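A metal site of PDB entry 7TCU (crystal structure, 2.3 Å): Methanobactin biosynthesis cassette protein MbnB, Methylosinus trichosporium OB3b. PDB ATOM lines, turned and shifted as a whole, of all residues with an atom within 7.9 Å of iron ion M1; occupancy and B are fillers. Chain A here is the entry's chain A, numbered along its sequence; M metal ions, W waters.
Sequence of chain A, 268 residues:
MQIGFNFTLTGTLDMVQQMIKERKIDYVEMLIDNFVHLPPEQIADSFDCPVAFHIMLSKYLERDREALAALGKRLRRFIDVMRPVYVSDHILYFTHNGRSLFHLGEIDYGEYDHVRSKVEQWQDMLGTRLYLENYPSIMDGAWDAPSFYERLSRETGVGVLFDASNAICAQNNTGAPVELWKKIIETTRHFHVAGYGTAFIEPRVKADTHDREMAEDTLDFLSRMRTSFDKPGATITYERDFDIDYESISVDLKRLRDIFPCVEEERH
Within 4 Å of iron ion M1: His 54, His 90 and Glu 133.
The nearest printed residue that does not touch iron ion M1 is His 192 (4.2 Å).
Iron ion M1 is bound by a ring nitrogen (NE2) of His 90 (2.0 Å), water W2 (2.1 Å), water W1 (2.1 Å), a ring nitrogen (NE2) of His 54 (2.2 Å), water W3 (2.4 Å) and the side-chain carboxylate of Glu 133 (2.4 Å).
ND1 of His 90 lies within hydrogen-bond range of O of Ile 55, 3.0 Å away.
ND1 of His 54 sits at hydrogen-bond distance from OG of Ser 88 (2.7 Å).
The backbone NH of Glu 133 is in hydrogen-bond range of the backbone carbonyl oxygen of Asp 89, 3.0 Å away.
The side-chain carboxylate of Glu 133 is in hydrogen-bond range of the side-chain amide nitrogen of Asn 166, 3.4 Å away.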
ATOM      1  N   ASN A   6     -22.770 -19.456 -19.444  1.00  0.00           N
ATOM      2  CA  ASN A   6     -22.563 -19.526 -20.884  1.00  0.00           C
ATOM      3  C   ASN A   6     -21.319 -20.352 -21.189  1.00  0.00           C
ATOM      4  O   ASN A   6     -20.237 -20.100 -20.647  1.00  0.00           O
ATOM      5  CB  ASN A   6     -22.477 -18.125 -21.510  1.00  0.00           C
ATOM      6  CG  ASN A   6     -21.145 -17.394 -21.246  1.00  0.00           C
ATOM      7  OD1 ASN A   6     -20.651 -17.342 -20.117  1.00  0.00           O
ATOM      8  ND2 ASN A   6     -20.582 -16.809 -22.303  1.00  0.00           N
ATOM      9  N   GLU A  29     -26.069 -22.388 -21.232  1.00  0.00           N
ATOM     10  CA  GLU A  29     -26.342 -21.729 -22.497  1.00  0.00           C
ATOM     11  C   GLU A  29     -25.091 -21.810 -23.343  1.00  0.00           C
ATOM     12  O   GLU A  29     -24.060 -21.218 -22.995  1.00  0.00           O
ATOM     13  CB  GLU A  29     -26.752 -20.272 -22.288  1.00  0.00           C
ATOM     14  CG  GLU A  29     -27.142 -19.520 -23.550  1.00  0.00           C
ATOM     15  CD  GLU A  29     -27.454 -18.043 -23.239  1.00  0.00           C
ATOM     16  OE1 GLU A  29     -28.403 -17.781 -22.437  1.00  0.00           O
ATOM     17  OE2 GLU A  29     -26.719 -17.161 -23.736  1.00  0.00           O
ATOM     18  N   LEU A  31     -22.855 -21.146 -26.797  1.00  0.00           N
ATOM     19  CA  LEU A  31     -22.619 -20.381 -28.018  1.00  0.00           C
ATOM     20  C   LEU A  31     -22.535 -21.398 -29.143  1.00  0.00           C
ATOM     21  O   LEU A  31     -21.457 -21.808 -29.601  1.00  0.00           O
ATOM     22  CB  LEU A  31     -21.369 -19.536 -27.877  1.00  0.00           C
ATOM     23  CG  LEU A  31     -21.342 -18.275 -28.732  1.00  0.00           C
ATOM     24  CD1 LEU A  31     -22.130 -17.154 -28.036  1.00  0.00           C
ATOM     25  CD2 LEU A  31     -19.908 -17.876 -28.926  1.00  0.00           C
ATOM     26  N   HIS A  54     -27.338 -19.887 -27.873  1.00  0.00           N
ATOM     27  CA  HIS A  54     -26.983 -18.536 -28.258  1.00  0.00           C
ATOM     28  C   HIS A  54     -26.158 -18.596 -29.546  1.00  0.00           C
ATOM     29  O   HIS A  54     -25.160 -19.312 -29.605  1.00  0.00           O
ATOM     30  CB  HIS A  54     -26.171 -17.853 -27.143  1.00  0.00           C
ATOM     31  CG  HIS A  54     -26.266 -16.363 -27.123  1.00  0.00           C
ATOM     32  ND1 HIS A  54     -27.438 -15.690 -27.372  1.00  0.00           N
ATOM     33  CD2 HIS A  54     -25.343 -15.419 -26.836  1.00  0.00           C
ATOM     34  CE1 HIS A  54     -27.230 -14.391 -27.274  1.00  0.00           C
ATOM     35  NE2 HIS A  54     -25.964 -14.198 -26.939  1.00  0.00           N
ATOM     36  N   ILE A  55     -26.577 -17.869 -30.578  1.00  0.00           N
ATOM     37  CA  ILE A  55     -25.903 -17.892 -31.877  1.00  0.00           C
ATOM     38  C   ILE A  55     -25.171 -16.563 -32.060  1.00  0.00           C
ATOM     39  O   ILE A  55     -25.785 -15.498 -32.012  1.00  0.00           O
ATOM     40  CB  ILE A  55     -26.906 -18.138 -33.019  1.00  0.00           C
ATOM     41  CG1 ILE A  55     -27.567 -19.505 -32.841  1.00  0.00           C
ATOM     42  CG2 ILE A  55     -26.242 -18.013 -34.368  1.00  0.00           C
ATOM     43  CD1 ILE A  55     -29.032 -19.519 -33.271  1.00  0.00           C
ATOM     44  N   MET A  56     -23.863 -16.624 -32.292  1.00  0.00           N
ATOM     45  CA  MET A  56     -23.121 -15.374 -32.338  1.00  0.00           C
ATOM     46  C   MET A  56     -22.779 -14.917 -33.744  1.00  0.00           C
ATOM     47  O   MET A  56     -22.799 -13.711 -34.010  1.00  0.00           O
ATOM     48  CB  MET A  56     -21.830 -15.498 -31.508  1.00  0.00           C
ATOM     49  CG  MET A  56     -20.929 -14.249 -31.513  1.00  0.00           C
ATOM     50  SD  MET A  56     -21.602 -12.835 -30.560  1.00  0.00           S
ATOM     51  CE  MET A  56     -20.890 -11.500 -31.501  1.00  0.00           C
ATOM     52  N   SER A  88     -31.399 -18.169 -29.499  1.00  0.00           N
ATOM     53  CA  SER A  88     -31.194 -16.728 -29.462  1.00  0.00           C
ATOM     54  C   SER A  88     -30.039 -16.308 -30.356  1.00  0.00           C
ATOM     55  O   SER A  88     -29.135 -17.098 -30.673  1.00  0.00           O
ATOM     56  CB  SER A  88     -30.940 -16.222 -28.040  1.00  0.00           C
ATOM     57  OG  SER A  88     -29.840 -16.875 -27.432  1.00  0.00           O
ATOM     58  N   ASP A  89     -30.103 -15.045 -30.755  1.00  0.00           N
ATOM     59  CA  ASP A  89     -29.170 -14.427 -31.679  1.00  0.00           C
ATOM     60  C   ASP A  89     -29.128 -12.924 -31.371  1.00  0.00           C
ATOM     61  O   ASP A  89     -29.644 -12.473 -30.337  1.00  0.00           O
ATOM     62  CB  ASP A  89     -29.607 -14.747 -33.111  1.00  0.00           C
ATOM     63  CG  ASP A  89     -28.463 -14.763 -34.103  1.00  0.00           C
ATOM     64  OD1 ASP A  89     -27.658 -13.810 -34.150  1.00  0.00           O
ATOM     65  OD2 ASP A  89     -28.408 -15.701 -34.905  1.00  0.00           O
ATOM     66  N   HIS A  90     -28.531 -12.153 -32.272  1.00  0.00           N
ATOM     67  CA  HIS A  90     -28.189 -10.771 -32.024  1.00  0.00           C
ATOM     68  C   HIS A  90     -28.683  -9.861 -33.133  1.00  0.00           C
ATOM     69  O   HIS A  90     -29.147 -10.320 -34.177  1.00  0.00           O
ATOM     70  CB  HIS A  90     -26.679 -10.600 -31.895  1.00  0.00           C
ATOM     71  CG  HIS A  90     -26.068 -11.374 -30.779  1.00  0.00           C
ATOM     72  ND1 HIS A  90     -25.849 -12.737 -30.855  1.00  0.00           N
ATOM     73  CD2 HIS A  90     -25.671 -10.982 -29.548  1.00  0.00           C
ATOM     74  CE1 HIS A  90     -25.313 -13.144 -29.713  1.00  0.00           C
ATOM     75  NE2 HIS A  90     -25.185 -12.099 -28.907  1.00  0.00           N
ATOM     76  N   LEU A  92     -26.555  -7.085 -34.879  1.00  0.00           N
ATOM     77  CA  LEU A  92     -25.197  -6.569 -34.866  1.00  0.00           C
ATOM     78  C   LEU A  92     -24.782  -6.173 -36.272  1.00  0.00           C
ATOM     79  O   LEU A  92     -25.169  -6.797 -37.256  1.00  0.00           O
ATOM     80  CB  LEU A  92     -24.216  -7.618 -34.293  1.00  0.00           C
ATOM     81  CG  LEU A  92     -24.329  -7.894 -32.801  1.00  0.00           C
ATOM     82  CD1 LEU A  92     -23.438  -9.065 -32.476  1.00  0.00           C
ATOM     83  CD2 LEU A  92     -23.902  -6.689 -32.013  1.00  0.00           C
ATOM     84  N   GLU A 133     -31.163 -10.325 -28.819  1.00  0.00           N
ATOM     85  CA  GLU A 133     -30.526  -9.645 -27.715  1.00  0.00           C
ATOM     86  C   GLU A 133     -30.406  -8.144 -27.977  1.00  0.00           C
ATOM     87  O   GLU A 133     -30.287  -7.698 -29.123  1.00  0.00           O
ATOM     88  CB  GLU A 133     -29.135 -10.250 -27.520  1.00  0.00           C
ATOM     89  CG  GLU A 133     -28.324  -9.762 -26.335  1.00  0.00           C
ATOM     90  CD  GLU A 133     -26.971 -10.474 -26.280  1.00  0.00           C
ATOM     91  OE1 GLU A 133     -26.942 -11.718 -26.300  1.00  0.00           O
ATOM     92  OE2 GLU A 133     -25.918  -9.796 -26.250  1.00  0.00           O
ATOM     93  N   ASN A 134     -30.447  -7.356 -26.900  1.00  0.00           N
ATOM     94  CA  ASN A 134     -30.184  -5.920 -27.025  1.00  0.00           C
ATOM     95  C   ASN A 134     -28.690  -5.634 -26.984  1.00  0.00           C
ATOM     96  O   ASN A 134     -27.903  -6.321 -26.311  1.00  0.00           O
ATOM     97  CB  ASN A 134     -30.881  -5.116 -25.923  1.00  0.00           C
ATOM     98  CG  ASN A 134     -30.629  -5.702 -24.540  1.00  0.00           C
ATOM     99  OD1 ASN A 134     -30.881  -6.897 -24.309  1.00  0.00           O
ATOM    100  ND2 ASN A 134     -30.115  -4.874 -23.626  1.00  0.00           N
ATOM    101  N   LEU A 161     -34.188 -11.480 -25.810  1.00  0.00           N
ATOM    102  CA  LEU A 161     -33.280 -12.005 -24.805  1.00  0.00           C
ATOM    103  C   LEU A 161     -32.694 -10.771 -24.135  1.00  0.00           C
ATOM    104  O   LEU A 161     -31.730 -10.190 -24.614  1.00  0.00           O
ATOM    105  CB  LEU A 161     -32.218 -12.875 -25.439  1.00  0.00           C
ATOM    106  CG  LEU A 161     -31.210 -13.442 -24.448  1.00  0.00           C
ATOM    107  CD1 LEU A 161     -31.946 -14.015 -23.276  1.00  0.00           C
ATOM    108  CD2 LEU A 161     -30.366 -14.505 -25.127  1.00  0.00           C
ATOM    109  N   ASP A 163     -30.630  -8.505 -22.098  1.00  0.00           N
ATOM    110  CA  ASP A 163     -29.325  -8.480 -21.439  1.00  0.00           C
ATOM    111  C   ASP A 163     -29.270  -7.279 -20.500  1.00  0.00           C
ATOM    112  O   ASP A 163     -29.144  -6.138 -20.945  1.00  0.00           O
ATOM    113  CB  ASP A 163     -28.218  -8.438 -22.481  1.00  0.00           C
ATOM    114  CG  ASP A 163     -26.820  -8.707 -21.862  1.00  0.00           C
ATOM    115  OD1 ASP A 163     -26.362  -7.875 -21.033  1.00  0.00           O
ATOM    116  OD2 ASP A 163     -26.164  -9.726 -22.204  1.00  0.00           O
ATOM    117  N   ASN A 166     -25.955  -5.049 -20.602  1.00  0.00           N
ATOM    118  CA  ASN A 166     -25.923  -4.226 -21.812  1.00  0.00           C
ATOM    119  C   ASN A 166     -26.853  -3.020 -21.681  1.00  0.00           C
ATOM    120  O   ASN A 166     -26.504  -1.918 -22.111  1.00  0.00           O
ATOM    121  CB  ASN A 166     -26.326  -5.059 -23.029  1.00  0.00           C
ATOM    122  CG  ASN A 166     -25.325  -6.152 -23.326  1.00  0.00           C
ATOM    123  OD1 ASN A 166     -24.345  -6.311 -22.615  1.00  0.00           O
ATOM    124  ND2 ASN A 166     -25.586  -6.925 -24.366  1.00  0.00           N
ATOM    125  N   HIS A 192     -30.045 -12.144 -19.674  1.00  0.00           N
ATOM    126  CA  HIS A 192     -28.583 -12.314 -19.624  1.00  0.00           C
ATOM    127  C   HIS A 192     -28.048 -11.265 -18.659  1.00  0.00           C
ATOM    128  O   HIS A 192     -28.666 -10.213 -18.553  1.00  0.00           O
ATOM    129  CB  HIS A 192     -27.972 -11.915 -20.945  1.00  0.00           C
ATOM    130  CG  HIS A 192     -27.760 -12.996 -21.923  1.00  0.00           C
ATOM    131  ND1 HIS A 192     -26.933 -12.815 -23.003  1.00  0.00           N
ATOM    132  CD2 HIS A 192     -28.258 -14.233 -22.004  1.00  0.00           C
ATOM    133  CE1 HIS A 192     -26.923 -13.919 -23.722  1.00  0.00           C
ATOM    134  NE2 HIS A 192     -27.749 -14.780 -23.132  1.00  0.00           N
ATOM    135  N   ASP A 208     -18.824  -3.892 -22.850  1.00  0.00           N
ATOM    136  CA  ASP A 208     -19.402  -5.204 -22.480  1.00  0.00           C
ATOM    137  C   ASP A 208     -18.324  -6.299 -22.496  1.00  0.00           C
ATOM    138  O   ASP A 208     -18.318  -7.228 -23.319  1.00  0.00           O
ATOM    139  CB  ASP A 208     -20.572  -5.539 -23.405  1.00  0.00           C
ATOM    140  CG  ASP A 208     -20.148  -5.742 -24.863  1.00  0.00           C
ATOM    141  OD1 ASP A 208     -19.588  -4.807 -25.482  1.00  0.00           O
ATOM    142  OD2 ASP A 208     -20.384  -6.832 -25.408  1.00  0.00           O
ATOM    143  N   HIS A 210     -17.524  -8.681 -20.240  1.00  0.00           N
ATOM    144  CA  HIS A 210     -17.849  -9.990 -19.649  1.00  0.00           C
ATOM    145  C   HIS A 210     -16.666 -10.591 -18.901  1.00  0.00           C
ATOM    146  O   HIS A 210     -16.459 -11.817 -18.916  1.00  0.00           O
ATOM    147  CB  HIS A 210     -18.352 -10.965 -20.708  1.00  0.00           C
ATOM    148  CG  HIS A 210     -19.589 -10.505 -21.408  1.00  0.00           C
ATOM    149  ND1 HIS A 210     -20.318 -11.319 -22.240  1.00  0.00           N
ATOM    150  CD2 HIS A 210     -20.216  -9.308 -21.404  1.00  0.00           C
ATOM    151  CE1 HIS A 210     -21.350 -10.646 -22.716  1.00  0.00           C
ATOM    152  NE2 HIS A 210     -21.306  -9.416 -22.233  1.00  0.00           N
ATOM    153  N   GLU A 239     -22.832 -14.532 -17.720  1.00  0.00           N
ATOM    154  CA  GLU A 239     -21.857 -14.688 -18.805  1.00  0.00           C
ATOM    155  C   GLU A 239     -20.468 -14.240 -18.375  1.00  0.00           C
ATOM    156  O   GLU A 239     -20.332 -13.114 -17.920  1.00  0.00           O
ATOM    157  CB  GLU A 239     -22.247 -13.872 -20.022  1.00  0.00           C
ATOM    158  CG  GLU A 239     -23.627 -14.186 -20.555  1.00  0.00           C
ATOM    159  CD  GLU A 239     -23.821 -13.597 -21.944  1.00  0.00           C
ATOM    160  OE1 GLU A 239     -24.044 -12.387 -22.035  1.00  0.00           O
ATOM    161  OE2 GLU A 239     -23.718 -14.363 -22.920  1.00  0.00           O
ATOM    162  N   ASP A 241     -16.652 -14.404 -20.215  1.00  0.00           N
ATOM    163  CA  ASP A 241     -15.839 -14.827 -21.338  1.00  0.00           C
ATOM    164  C   ASP A 241     -14.361 -14.664 -21.079  1.00  0.00           C
ATOM    165  O   ASP A 241     -13.543 -15.244 -21.796  1.00  0.00           O
ATOM    166  CB  ASP A 241     -16.208 -14.016 -22.585  1.00  0.00           C
ATOM    167  CG  ASP A 241     -17.703 -13.999 -22.836  1.00  0.00           C
ATOM    168  OD1 ASP A 241     -18.352 -15.063 -22.753  1.00  0.00           O
ATOM    169  OD2 ASP A 241     -18.243 -12.910 -23.117  1.00  0.00           O
HETATM  170 FE    FE M   1     -24.739 -12.327 -26.960  1.00  0.00          FE
HETATM  171 FE    FE M   2     -25.545 -10.980 -23.556  1.00  0.00          FE
HETATM  172 FE    FE M   3     -23.210  -8.118 -22.037  1.00  0.00          FE
HETATM  173  O   HOH W   1     -23.941 -12.404 -24.979  1.00  0.00           O
HETATM  174  O   HOH W   2     -23.735 -10.463 -26.924  1.00  0.00           O
HETATM  175  O   HOH W   3     -22.840 -13.478 -27.770  1.00  0.00           O
